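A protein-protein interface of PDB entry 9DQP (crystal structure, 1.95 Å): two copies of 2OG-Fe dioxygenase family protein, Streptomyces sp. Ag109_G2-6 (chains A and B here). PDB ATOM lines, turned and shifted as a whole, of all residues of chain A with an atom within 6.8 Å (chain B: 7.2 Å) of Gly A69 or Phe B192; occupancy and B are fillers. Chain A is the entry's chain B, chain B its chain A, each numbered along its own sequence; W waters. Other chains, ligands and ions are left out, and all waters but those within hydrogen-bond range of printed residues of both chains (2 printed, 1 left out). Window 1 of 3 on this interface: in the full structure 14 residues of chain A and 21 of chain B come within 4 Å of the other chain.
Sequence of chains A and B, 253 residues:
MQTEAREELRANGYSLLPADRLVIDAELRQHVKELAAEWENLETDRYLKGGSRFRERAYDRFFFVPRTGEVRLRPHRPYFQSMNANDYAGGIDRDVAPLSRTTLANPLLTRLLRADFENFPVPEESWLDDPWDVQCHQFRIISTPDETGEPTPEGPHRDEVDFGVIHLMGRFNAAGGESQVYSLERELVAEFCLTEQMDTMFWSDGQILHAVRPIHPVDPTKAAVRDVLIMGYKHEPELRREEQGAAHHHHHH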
ATOM      1  N   PHE A  63     -12.419 -21.964 -27.232  1.00  0.00           N
ATOM      2  CA  PHE A  63     -13.607 -21.404 -27.851  1.00  0.00           C
ATOM      3  C   PHE A  63     -13.332 -19.925 -28.114  1.00  0.00           C
ATOM      4  O   PHE A  63     -12.926 -19.205 -27.200  1.00  0.00           O
ATOM      5  CB  PHE A  63     -14.775 -21.590 -26.875  1.00  0.00           C
ATOM      6  CG  PHE A  63     -16.092 -20.968 -27.301  1.00  0.00           C
ATOM      7  CD1 PHE A  63     -16.361 -19.627 -27.048  1.00  0.00           C
ATOM      8  CD2 PHE A  63     -17.100 -21.757 -27.841  1.00  0.00           C
ATOM      9  CE1 PHE A  63     -17.575 -19.070 -27.379  1.00  0.00           C
ATOM     10  CE2 PHE A  63     -18.332 -21.210 -28.166  1.00  0.00           C
ATOM     11  CZ  PHE A  63     -18.569 -19.861 -27.935  1.00  0.00           C
ATOM     12  N   PHE A  64     -13.550 -19.470 -29.348  1.00  0.00           N
ATOM     13  CA  PHE A  64     -13.195 -18.110 -29.736  1.00  0.00           C
ATOM     14  C   PHE A  64     -14.307 -17.506 -30.579  1.00  0.00           C
ATOM     15  O   PHE A  64     -14.751 -18.120 -31.550  1.00  0.00           O
ATOM     16  CB  PHE A  64     -11.852 -18.134 -30.498  1.00  0.00           C
ATOM     17  CG  PHE A  64     -11.484 -16.841 -31.169  1.00  0.00           C
ATOM     18  CD1 PHE A  64     -11.501 -15.648 -30.471  1.00  0.00           C
ATOM     19  CD2 PHE A  64     -11.049 -16.837 -32.485  1.00  0.00           C
ATOM     20  CE1 PHE A  64     -11.132 -14.470 -31.085  1.00  0.00           C
ATOM     21  CE2 PHE A  64     -10.673 -15.645 -33.114  1.00  0.00           C
ATOM     22  CZ  PHE A  64     -10.713 -14.472 -32.414  1.00  0.00           C
ATOM     23  N   VAL A  65     -14.774 -16.303 -30.216  1.00  0.00           N
ATOM     24  CA  VAL A  65     -15.707 -15.559 -31.034  1.00  0.00           C
ATOM     25  C   VAL A  65     -15.011 -14.255 -31.440  1.00  0.00           C
ATOM     26  O   VAL A  65     -14.671 -13.446 -30.585  1.00  0.00           O
ATOM     27  CB  VAL A  65     -17.049 -15.256 -30.314  1.00  0.00           C
ATOM     28  CG1 VAL A  65     -18.004 -14.486 -31.244  1.00  0.00           C
ATOM     29  CG2 VAL A  65     -17.733 -16.568 -29.830  1.00  0.00           C
ATOM     30  N   PRO A  66     -14.732 -14.052 -32.729  1.00  0.00           N
ATOM     31  CA  PRO A  66     -13.920 -12.881 -33.098  1.00  0.00           C
ATOM     32  C   PRO A  66     -14.552 -11.539 -32.780  1.00  0.00           C
ATOM     33  O   PRO A  66     -13.830 -10.613 -32.385  1.00  0.00           O
ATOM     34  CB  PRO A  66     -13.724 -13.085 -34.605  1.00  0.00           C
ATOM     35  CG  PRO A  66     -13.663 -14.559 -34.737  1.00  0.00           C
ATOM     36  CD  PRO A  66     -14.745 -15.060 -33.800  1.00  0.00           C
ATOM     37  N   ARG A  67     -15.870 -11.390 -32.933  1.00  0.00           N
ATOM     38  CA  ARG A  67     -16.474 -10.066 -32.799  1.00  0.00           C
ATOM     39  C   ARG A  67     -16.256  -9.506 -31.403  1.00  0.00           C
ATOM     40  O   ARG A  67     -15.870  -8.343 -31.231  1.00  0.00           O
ATOM     41  CB  ARG A  67     -17.969 -10.113 -33.126  1.00  0.00           C
ATOM     42  CG  ARG A  67     -18.690  -8.762 -32.870  1.00  0.00           C
ATOM     43  CD  ARG A  67     -17.965  -7.570 -33.520  1.00  0.00           C
ATOM     44  NE  ARG A  67     -18.627  -6.298 -33.222  1.00  0.00           N
ATOM     45  CZ  ARG A  67     -18.384  -5.536 -32.162  1.00  0.00           C
ATOM     46  NH1 ARG A  67     -17.413  -5.825 -31.303  1.00  0.00           N
ATOM     47  NH2 ARG A  67     -19.148  -4.464 -31.948  1.00  0.00           N
ATOM     48  N   THR A  68     -16.481 -10.331 -30.397  1.00  0.00           N
ATOM     49  CA  THR A  68     -16.362  -9.934 -29.013  1.00  0.00           C
ATOM     50  C   THR A  68     -14.988 -10.212 -28.441  1.00  0.00           C
ATOM     51  O   THR A  68     -14.706  -9.784 -27.322  1.00  0.00           O
ATOM     52  CB  THR A  68     -17.392 -10.700 -28.175  1.00  0.00           C
ATOM     53  OG1 THR A  68     -17.144 -12.098 -28.347  1.00  0.00           O
ATOM     54  CG2 THR A  68     -18.826 -10.384 -28.629  1.00  0.00           C
ATOM     55  N   GLY A  69     -14.145 -10.950 -29.164  1.00  0.00           N
ATOM     56  CA  GLY A  69     -12.901 -11.405 -28.597  1.00  0.00           C
ATOM     57  C   GLY A  69     -13.051 -12.467 -27.534  1.00  0.00           C
ATOM     58  O   GLY A  69     -12.083 -12.751 -26.841  1.00  0.00           O
ATOM     59  N   GLU A  70     -14.245 -13.038 -27.348  1.00  0.00           N
ATOM     60  CA  GLU A  70     -14.415 -14.031 -26.299  1.00  0.00           C
ATOM     61  C   GLU A  70     -13.482 -15.212 -26.549  1.00  0.00           C
ATOM     62  O   GLU A  70     -13.404 -15.725 -27.666  1.00  0.00           O
ATOM     63  CB  GLU A  70     -15.864 -14.498 -26.244  1.00  0.00           C
ATOM     64  CG  GLU A  70     -16.127 -15.504 -25.129  1.00  0.00           C
ATOM     65  CD  GLU A  70     -17.585 -15.953 -25.071  1.00  0.00           C
ATOM     66  OE1 GLU A  70     -18.326 -15.713 -26.042  1.00  0.00           O
ATOM     67  OE2 GLU A  70     -17.981 -16.546 -24.048  1.00  0.00           O
ATOM     68  N   VAL A  71     -12.731 -15.595 -25.514  1.00  0.00           N
ATOM     69  CA  VAL A  71     -11.816 -16.735 -25.532  1.00  0.00           C
ATOM     70  C   VAL A  71     -12.074 -17.521 -24.256  1.00  0.00           C
ATOM     71  O   VAL A  71     -12.032 -16.953 -23.160  1.00  0.00           O
ATOM     72  CB  VAL A  71     -10.340 -16.287 -25.607  1.00  0.00           C
ATOM     73  CG1 VAL A  71      -9.392 -17.479 -25.495  1.00  0.00           C
ATOM     74  CG2 VAL A  71     -10.072 -15.548 -26.919  1.00  0.00           C
ATOM     75  N   ARG A  72     -12.382 -18.812 -24.394  1.00  0.00           N
ATOM     76  CA  ARG A  72     -12.626 -19.713 -23.275  1.00  0.00           C
ATOM     77  C   ARG A  72     -11.757 -20.945 -23.473  1.00  0.00           C
ATOM     78  O   ARG A  72     -11.828 -21.580 -24.522  1.00  0.00           O
ATOM     79  CB  ARG A  72     -14.101 -20.156 -23.197  1.00  0.00           C
ATOM     80  CG  ARG A  72     -15.137 -19.040 -23.094  1.00  0.00           C
ATOM     81  CD  ARG A  72     -16.548 -19.606 -23.317  1.00  0.00           C
ATOM     82  NE  ARG A  72     -16.819 -20.729 -22.427  1.00  0.00           N
ATOM     83  CZ  ARG A  72     -17.361 -20.629 -21.223  1.00  0.00           C
ATOM     84  NH1 ARG A  72     -17.707 -19.460 -20.711  1.00  0.00           N
ATOM     85  NH2 ARG A  72     -17.569 -21.733 -20.515  1.00  0.00           N
ATOM     86  N   LEU A 113      -3.485 -14.798 -30.133  1.00  0.00           N
ATOM     87  CA  LEU A 113      -4.646 -15.484 -30.688  1.00  0.00           C
ATOM     88  C   LEU A 113      -5.564 -14.496 -31.404  1.00  0.00           C
ATOM     89  O   LEU A 113      -5.942 -14.721 -32.554  1.00  0.00           O
ATOM     90  CB  LEU A 113      -5.389 -16.254 -29.585  1.00  0.00           C
ATOM     91  CG  LEU A 113      -6.544 -17.171 -30.043  1.00  0.00           C
ATOM     92  CD1 LEU A 113      -6.767 -18.332 -29.083  1.00  0.00           C
ATOM     93  CD2 LEU A 113      -7.879 -16.405 -30.220  1.00  0.00           C
ATOM     94  N   ARG A 114      -5.922 -13.377 -30.749  1.00  0.00           N
ATOM     95  CA  ARG A 114      -6.848 -12.432 -31.382  1.00  0.00           C
ATOM     96  C   ARG A 114      -6.171 -11.674 -32.517  1.00  0.00           C
ATOM     97  O   ARG A 114      -6.749 -11.485 -33.595  1.00  0.00           O
ATOM     98  CB  ARG A 114      -7.398 -11.438 -30.347  1.00  0.00           C
ATOM     99  CG  ARG A 114      -8.190 -12.105 -29.199  1.00  0.00           C
ATOM    100  CD  ARG A 114      -8.877 -11.042 -28.309  1.00  0.00           C
ATOM    101  NE  ARG A 114      -9.497 -11.671 -27.143  1.00  0.00           N
ATOM    102  CZ  ARG A 114      -8.885 -11.842 -25.982  1.00  0.00           C
ATOM    103  NH1 ARG A 114      -7.658 -11.382 -25.774  1.00  0.00           N
ATOM    104  NH2 ARG A 114      -9.499 -12.532 -25.023  1.00  0.00           N
ATOM    105  N   TYR B  14     -22.291 -15.004 -17.482  1.00  0.00           N
ATOM    106  CA  TYR B  14     -22.095 -13.745 -18.204  1.00  0.00           C
ATOM    107  C   TYR B  14     -22.611 -13.918 -19.622  1.00  0.00           C
ATOM    108  O   TYR B  14     -22.800 -15.038 -20.097  1.00  0.00           O
ATOM    109  CB  TYR B  14     -20.615 -13.316 -18.215  1.00  0.00           C
ATOM    110  CG  TYR B  14     -19.790 -14.194 -19.121  1.00  0.00           C
ATOM    111  CD1 TYR B  14     -19.358 -15.440 -18.695  1.00  0.00           C
ATOM    112  CD2 TYR B  14     -19.466 -13.786 -20.417  1.00  0.00           C
ATOM    113  CE1 TYR B  14     -18.620 -16.262 -19.520  1.00  0.00           C
ATOM    114  CE2 TYR B  14     -18.714 -14.614 -21.259  1.00  0.00           C
ATOM    115  CZ  TYR B  14     -18.312 -15.853 -20.800  1.00  0.00           C
ATOM    116  OH  TYR B  14     -17.590 -16.695 -21.627  1.00  0.00           O
ATOM    117  N   SER B  15     -22.832 -12.792 -20.304  1.00  0.00           N
ATOM    118  CA  SER B  15     -23.345 -12.785 -21.661  1.00  0.00           C
ATOM    119  C   SER B  15     -22.843 -11.512 -22.322  1.00  0.00           C
ATOM    120  O   SER B  15     -22.784 -10.471 -21.675  1.00  0.00           O
ATOM    121  CB  SER B  15     -24.891 -12.819 -21.684  1.00  0.00           C
ATOM    122  OG  SER B  15     -25.381 -12.843 -23.020  1.00  0.00           O
ATOM    123  N   LEU B  16     -22.462 -11.595 -23.589  1.00  0.00           N
ATOM    124  CA  LEU B  16     -21.880 -10.459 -24.293  1.00  0.00           C
ATOM    125  C   LEU B  16     -22.862  -9.958 -25.336  1.00  0.00           C
ATOM    126  O   LEU B  16     -23.607 -10.746 -25.922  1.00  0.00           O
ATOM    127  CB  LEU B  16     -20.541 -10.832 -24.962  1.00  0.00           C
ATOM    128  CG  LEU B  16     -19.554 -11.467 -23.993  1.00  0.00           C
ATOM    129  CD1 LEU B  16     -18.317 -12.015 -24.678  1.00  0.00           C
ATOM    130  CD2 LEU B  16     -19.158 -10.467 -22.920  1.00  0.00           C
ATOM    131  N   ILE B 166     -22.002  -3.750 -18.062  1.00  0.00           N
ATOM    132  CA  ILE B 166     -20.988  -2.767 -18.399  1.00  0.00           C
ATOM    133  C   ILE B 166     -21.162  -2.426 -19.861  1.00  0.00           C
ATOM    134  O   ILE B 166     -21.349  -3.324 -20.688  1.00  0.00           O
ATOM    135  CB  ILE B 166     -19.564  -3.274 -18.092  1.00  0.00           C
ATOM    136  CG1 ILE B 166     -18.506  -2.319 -18.655  1.00  0.00           C
ATOM    137  CG2 ILE B 166     -19.358  -4.685 -18.628  1.00  0.00           C
ATOM    138  CD1 ILE B 166     -17.113  -2.731 -18.238  1.00  0.00           C
ATOM    139  N   GLY B 176      -4.877  -3.566 -24.505  1.00  0.00           N
ATOM    140  CA  GLY B 176      -5.154  -4.193 -23.231  1.00  0.00           C
ATOM    141  C   GLY B 176      -6.595  -3.950 -22.819  1.00  0.00           C
ATOM    142  O   GLY B 176      -7.481  -3.736 -23.647  1.00  0.00           O
ATOM    143  N   GLY B 177      -6.826  -3.940 -21.510  1.00  0.00           N
ATOM    144  CA  GLY B 177      -8.182  -3.726 -21.047  1.00  0.00           C
ATOM    145  C   GLY B 177      -9.103  -4.905 -21.273  1.00  0.00           C
ATOM    146  O   GLY B 177     -10.316  -4.735 -21.263  1.00  0.00           O
ATOM    147  N   GLU B 178      -8.554  -6.093 -21.516  1.00  0.00           N
ATOM    148  CA  GLU B 178      -9.394  -7.274 -21.693  1.00  0.00           C
ATOM    149  C   GLU B 178     -10.163  -7.575 -20.406  1.00  0.00           C
ATOM    150  O   GLU B 178      -9.625  -7.453 -19.302  1.00  0.00           O
ATOM    151  CB  GLU B 178      -8.533  -8.482 -22.086  1.00  0.00           C
ATOM    152  CG  GLU B 178      -7.773  -8.307 -23.402  1.00  0.00           C
ATOM    153  CD  GLU B 178      -6.395  -7.689 -23.219  1.00  0.00           C
ATOM    154  OE1 GLU B 178      -6.139  -7.115 -22.152  1.00  0.00           O
ATOM    155  OE2 GLU B 178      -5.557  -7.776 -24.143  1.00  0.00           O
ATOM    156  N   SER B 179     -11.431  -7.955 -20.555  1.00  0.00           N
ATOM    157  CA  SER B 179     -12.276  -8.309 -19.418  1.00  0.00           C
ATOM    158  C   SER B 179     -12.120  -9.789 -19.137  1.00  0.00           C
ATOM    159  O   SER B 179     -12.048 -10.602 -20.067  1.00  0.00           O
ATOM    160  CB  SER B 179     -13.749  -7.990 -19.686  1.00  0.00           C
ATOM    161  OG  SER B 179     -13.933  -6.646 -20.117  1.00  0.00           O
ATOM    162  N   GLN B 180     -12.057 -10.135 -17.855  1.00  0.00           N
ATOM    163  CA  GLN B 180     -11.793 -11.506 -17.441  1.00  0.00           C
ATOM    164  C   GLN B 180     -12.896 -11.989 -16.512  1.00  0.00           C
ATOM    165  O   GLN B 180     -13.363 -11.246 -15.645  1.00  0.00           O
ATOM    166  CB  GLN B 180     -10.432 -11.618 -16.765  1.00  0.00           C
ATOM    167  CG  GLN B 180      -9.326 -11.049 -17.651  1.00  0.00           C
ATOM    168  CD  GLN B 180      -7.936 -11.374 -17.174  1.00  0.00           C
ATOM    169  OE1 GLN B 180      -7.545 -10.996 -16.071  1.00  0.00           O
ATOM    170  NE2 GLN B 180      -7.167 -12.068 -18.015  1.00  0.00           N
ATOM    171  N   VAL B 181     -13.329 -13.225 -16.744  1.00  0.00           N
ATOM    172  CA  VAL B 181     -14.354 -13.895 -15.958  1.00  0.00           C
ATOM    173  C   VAL B 181     -13.680 -15.055 -15.236  1.00  0.00           C
ATOM    174  O   VAL B 181     -12.963 -15.844 -15.861  1.00  0.00           O
ATOM    175  CB  VAL B 181     -15.497 -14.397 -16.854  1.00  0.00           C
ATOM    176  CG1 VAL B 181     -16.540 -15.185 -16.046  1.00  0.00           C
ATOM    177  CG2 VAL B 181     -16.140 -13.230 -17.616  1.00  0.00           C
ATOM    178  N   ALA B 190     -13.030 -17.304 -18.866  1.00  0.00           N
ATOM    179  CA  ALA B 190     -13.325 -16.572 -20.089  1.00  0.00           C
ATOM    180  C   ALA B 190     -12.622 -15.212 -20.073  1.00  0.00           C
ATOM    181  O   ALA B 190     -12.393 -14.630 -19.016  1.00  0.00           O
ATOM    182  CB  ALA B 190     -14.839 -16.394 -20.251  1.00  0.00           C
ATOM    183  N   GLU B 191     -12.287 -14.711 -21.259  1.00  0.00           N
ATOM    184  CA  GLU B 191     -11.756 -13.363 -21.395  1.00  0.00           C
ATOM    185  C   GLU B 191     -12.276 -12.812 -22.710  1.00  0.00           C
ATOM    186  O   GLU B 191     -12.281 -13.529 -23.707  1.00  0.00           O
ATOM    187  CB  GLU B 191     -10.218 -13.402 -21.356  1.00  0.00           C
ATOM    188  CG  GLU B 191      -9.494 -12.091 -21.506  1.00  0.00           C
ATOM    189  CD  GLU B 191      -7.983 -12.342 -21.587  1.00  0.00           C
ATOM    190  OE1 GLU B 191      -7.519 -12.856 -22.629  1.00  0.00           O
ATOM    191  OE2 GLU B 191      -7.282 -12.069 -20.593  1.00  0.00           O
ATOM    192  N   PHE B 192     -12.720 -11.561 -22.716  1.00  0.00           N
ATOM    193  CA  PHE B 192     -13.232 -10.952 -23.936  1.00  0.00           C
ATOM    194  C   PHE B 192     -12.765  -9.503 -23.958  1.00  0.00           C
ATOM    195  O   PHE B 192     -12.149  -9.022 -23.006  1.00  0.00           O
ATOM    196  CB  PHE B 192     -14.759 -11.065 -24.013  1.00  0.00           C
ATOM    197  CG  PHE B 192     -15.449 -10.501 -22.822  1.00  0.00           C
ATOM    198  CD1 PHE B 192     -15.656 -11.273 -21.703  1.00  0.00           C
ATOM    199  CD2 PHE B 192     -15.837  -9.184 -22.798  1.00  0.00           C
ATOM    200  CE1 PHE B 192     -16.270 -10.736 -20.591  1.00  0.00           C
ATOM    201  CE2 PHE B 192     -16.443  -8.651 -21.682  1.00  0.00           C
ATOM    202  CZ  PHE B 192     -16.659  -9.427 -20.592  1.00  0.00           C
ATOM    203  N   CYS B 193     -13.117  -8.807 -25.046  1.00  0.00           N
ATOM    204  CA  CYS B 193     -12.660  -7.447 -25.312  1.00  0.00           C
ATOM    205  C   CYS B 193     -13.846  -6.577 -25.694  1.00  0.00           C
ATOM    206  O   CYS B 193     -14.439  -6.762 -26.760  1.00  0.00           O
ATOM    207  CB  CYS B 193     -11.628  -7.424 -26.441  1.00  0.00           C
ATOM    208  SG  CYS B 193     -10.205  -8.428 -26.127  1.00  0.00           S
ATOM    209  N   LEU B 194     -14.178  -5.606 -24.863  1.00  0.00           N
ATOM    210  CA  LEU B 194     -15.091  -4.580 -25.325  1.00  0.00           C
ATOM    211  C   LEU B 194     -14.291  -3.599 -26.171  1.00  0.00           C
ATOM    212  O   LEU B 194     -13.310  -3.021 -25.692  1.00  0.00           O
ATOM    213  CB  LEU B 194     -15.727  -3.887 -24.126  1.00  0.00           C
ATOM    214  CG  LEU B 194     -16.386  -4.827 -23.128  1.00  0.00           C
ATOM    215  CD1 LEU B 194     -16.751  -3.987 -21.928  1.00  0.00           C
ATOM    216  CD2 LEU B 194     -17.623  -5.487 -23.726  1.00  0.00           C
ATOM    217  N   THR B 195     -14.672  -3.435 -27.422  1.00  0.00           N
ATOM    218  CA  THR B 195     -13.822  -2.646 -28.298  1.00  0.00           C
ATOM    219  C   THR B 195     -14.581  -1.519 -28.979  1.00  0.00           C
ATOM    220  O   THR B 195     -14.004  -0.459 -29.209  1.00  0.00           O
ATOM    221  CB  THR B 195     -13.152  -3.537 -29.368  1.00  0.00           C
ATOM    222  OG1 THR B 195     -14.149  -4.337 -30.002  1.00  0.00           O
ATOM    223  CG2 THR B 195     -12.087  -4.448 -28.753  1.00  0.00           C
ATOM    224  N   THR B 200     -21.173  -4.469 -24.906  1.00  0.00           N
ATOM    225  CA  THR B 200     -21.828  -4.622 -23.609  1.00  0.00           C
ATOM    226  C   THR B 200     -21.551  -6.014 -23.059  1.00  0.00           C
ATOM    227  O   THR B 200     -21.447  -6.980 -23.816  1.00  0.00           O
ATOM    228  CB  THR B 200     -23.359  -4.381 -23.746  1.00  0.00           C
ATOM    229  OG1 THR B 200     -23.626  -2.997 -24.038  1.00  0.00           O
ATOM    230  CG2 THR B 200     -24.115  -4.763 -22.503  1.00  0.00           C
ATOM    231  N   MET B 201     -21.413  -6.107 -21.735  1.00  0.00           N
ATOM    232  CA  MET B 201     -21.422  -7.398 -21.049  1.00  0.00           C
ATOM    233  C   MET B 201     -22.409  -7.373 -19.892  1.00  0.00           C
ATOM    234  O   MET B 201     -22.467  -6.391 -19.146  1.00  0.00           O
ATOM    235  CB  MET B 201     -20.024  -7.771 -20.507  1.00  0.00           C
ATOM    236  CG  MET B 201     -19.987  -9.155 -19.845  1.00  0.00           C
ATOM    237  SD  MET B 201     -19.920  -9.020 -18.064  1.00  0.00           S
ATOM    238  CE  MET B 201     -18.380  -8.135 -17.809  1.00  0.00           C
ATOM    239  N   PHE B 202     -23.171  -8.464 -19.726  1.00  0.00           N
ATOM    240  CA  PHE B 202     -24.016  -8.683 -18.550  1.00  0.00           C
ATOM    241  C   PHE B 202     -23.414  -9.797 -17.697  1.00  0.00           C
ATOM    242  O   PHE B 202     -22.851 -10.748 -18.236  1.00  0.00           O
ATOM    243  CB  PHE B 202     -25.451  -9.088 -18.961  1.00  0.00           C
ATOM    244  CG  PHE B 202     -26.057  -8.234 -20.048  1.00  0.00           C
ATOM    245  CD1 PHE B 202     -26.665  -7.022 -19.742  1.00  0.00           C
ATOM    246  CD2 PHE B 202     -26.079  -8.675 -21.366  1.00  0.00           C
ATOM    247  CE1 PHE B 202     -27.233  -6.233 -20.748  1.00  0.00           C
ATOM    248  CE2 PHE B 202     -26.651  -7.901 -22.374  1.00  0.00           C
ATOM    249  CZ  PHE B 202     -27.225  -6.669 -22.063  1.00  0.00           C
ATOM    250  N   ALA B 211     -12.655  -9.275 -13.487  1.00  0.00           N
ATOM    251  CA  ALA B 211     -11.530  -8.361 -13.402  1.00  0.00           C
ATOM    252  C   ALA B 211     -11.317  -7.778 -14.784  1.00  0.00           C
ATOM    253  O   ALA B 211     -11.865  -8.265 -15.769  1.00  0.00           O
ATOM    254  CB  ALA B 211     -10.260  -9.074 -12.912  1.00  0.00           C
ATOM    255  N   VAL B 212     -10.509  -6.734 -14.852  1.00  0.00           N
ATOM    256  CA  VAL B 212     -10.163  -6.124 -16.132  1.00  0.00           C
ATOM    257  C   VAL B 212      -8.666  -5.862 -16.146  1.00  0.00           C
ATOM    258  O   VAL B 212      -8.108  -5.385 -15.154  1.00  0.00           O
ATOM    259  CB  VAL B 212     -10.969  -4.836 -16.391  1.00  0.00           C
ATOM    260  CG1 VAL B 212     -10.589  -3.724 -15.421  1.00  0.00           C
ATOM    261  CG2 VAL B 212     -10.796  -4.383 -17.843  1.00  0.00           C
ATOM    262  N   ARG B 226     -10.001   4.659 -21.412  1.00  0.00           N
ATOM    263  CA  ARG B 226     -11.098   3.697 -21.525  1.00  0.00           C
ATOM    264  C   ARG B 226     -12.280   4.217 -20.717  1.00  0.00           C
ATOM    265  O   ARG B 226     -12.157   4.423 -19.507  1.00  0.00           O
ATOM    266  CB  ARG B 226     -10.661   2.322 -21.017  1.00  0.00           C
ATOM    267  CG  ARG B 226     -11.700   1.186 -21.148  1.00  0.00           C
ATOM    268  CD  ARG B 226     -11.080  -0.141 -20.711  1.00  0.00           C
ATOM    269  NE  ARG B 226     -11.958  -1.290 -20.931  1.00  0.00           N
ATOM    270  CZ  ARG B 226     -12.776  -1.793 -20.018  1.00  0.00           C
ATOM    271  NH1 ARG B 226     -12.835  -1.294 -18.793  1.00  0.00           N
ATOM    272  NH2 ARG B 226     -13.561  -2.818 -20.347  1.00  0.00           N
HETATM  273  O   HOH W   1      -9.887 -17.146 -21.264  1.00  0.00           O
HETATM  274  O   HOH W   2      -6.154  -9.217 -26.954  1.00  0.00           O
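OH of Tyr B14 lies within hydrogen-bond range of OE2 of Glu A70 (2.5 Å). The backbone carbonyl oxygen (O) of Thr A68 lies within hydrogen-bond range of the backbone NH (N) of Cys B193 (2.9 Å). SG of Cys B193 is in hydrogen-bond range of NE of Arg A114, at 3.5 Å. O of Gly A69 lies close to O of Glu B191, 3.2 Å away. The backbone carbonyl oxygen (O) of Glu B191 sits at hydrogen-bond distance from the backbone NH (N) of Val A71. The guanidinium group (NH1) of Arg A72 sits at hydrogen-bond distance from the side-chain hydroxyl (OH) of Tyr B14. The side-chain carboxylate (OE1) of Glu B191 is in salt-bridge range of the guanidinium group (NH2) of Arg A114 (3.1 Å).
The backbone NH (N) of Val B181 sits at hydrogen-bond distance from the backbone carbonyl oxygen (O) of Ala B190 (2.8 Å). N of Ser B179 sits at hydrogen-bond distance from O of Phe B192 (2.8 Å). O of Glu A70 lies within hydrogen-bond range of N of Val A65 (3.0 Å). The guanidinium group of Arg A114 is in hydrogen-bond range of the backbone carbonyl oxygen of Gly A69, at 2.8 Å. The side-chain hydroxyl of Thr A68 lies close to the backbone NH of Glu A70 (3.2 Å). The side-chain carboxylate of Glu B191 sits at hydrogen-bond distance from the side-chain amide nitrogen of Gln B180.
Among the printed residues, merely in contact across the chains: Arg A67 with Thr B195 (3.8 Å), Thr A68 with Leu B16 (3.8 Å), Thr A68 with Phe B192 (3.5 Å), Gly A69 with Phe B192 (3.6 Å), Glu A70 with Leu B16 (3.8 Å), Glu A70 with Glu B191 (3.4 Å), Glu A70 with Phe B192 (3.8 Å), Val A71 with Ala B190 (3.4 Å), Arg A72 with Ala B190 (3.9 Å) and Arg A114 with Glu B178 (3.9 Å).
Printed residues of chain B within 4 Å of Thr A68: Leu B16 (3.8 Å), Phe B192 (3.5 Å) and Cys B193 (2.9 Å). Printed residues of chain B within 4 Å of Gly A69: Glu B191 (3.2 Å) and Phe B192 (3.6 Å). Of the printed residues of chain B, Arg A72 touches Tyr B14 (2.9 Å) and Ala B190 (3.9 Å). Printed residues of chain A within 4 Å of Ala B190: Val A71 and Arg A72. Printed residues of chain A within 4 Å of Glu B191: Gly A69 (3.2 Å), Glu A70 (3.4 Å), Val A71 (2.8 Å) and Arg A114 (3.1 Å). Of chain A, only Thr A68, Gly A69 and Glu A70 come within 4 Å of Phe B192. Printed residues of chain A within 4 Å of Thr B195: Arg A67 (3.8 Å).
Hydrophobic or aromatic side chains of chain A within 4 Å of the printed part of chain B: Val A71. Hydrophobic or aromatic side chains of chain B that line the printed part of chain A: Tyr B14, Leu B16, Ala B190 and Phe B192. Among the printed residues, Asp or Glu carboxylates within 4 Å of a Lys or Arg side-chain nitrogen of the other chain: Arg A114 with Glu B191.
No position is printed for both chains.
Water W1 lies within hydrogen-bond range of O of Val A71 (2.9 Å) and N of Glu B191 (3.4 Å). Water W2 lies within hydrogen-bond range of NH1 of Arg A114 and OE2 of Glu B178.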
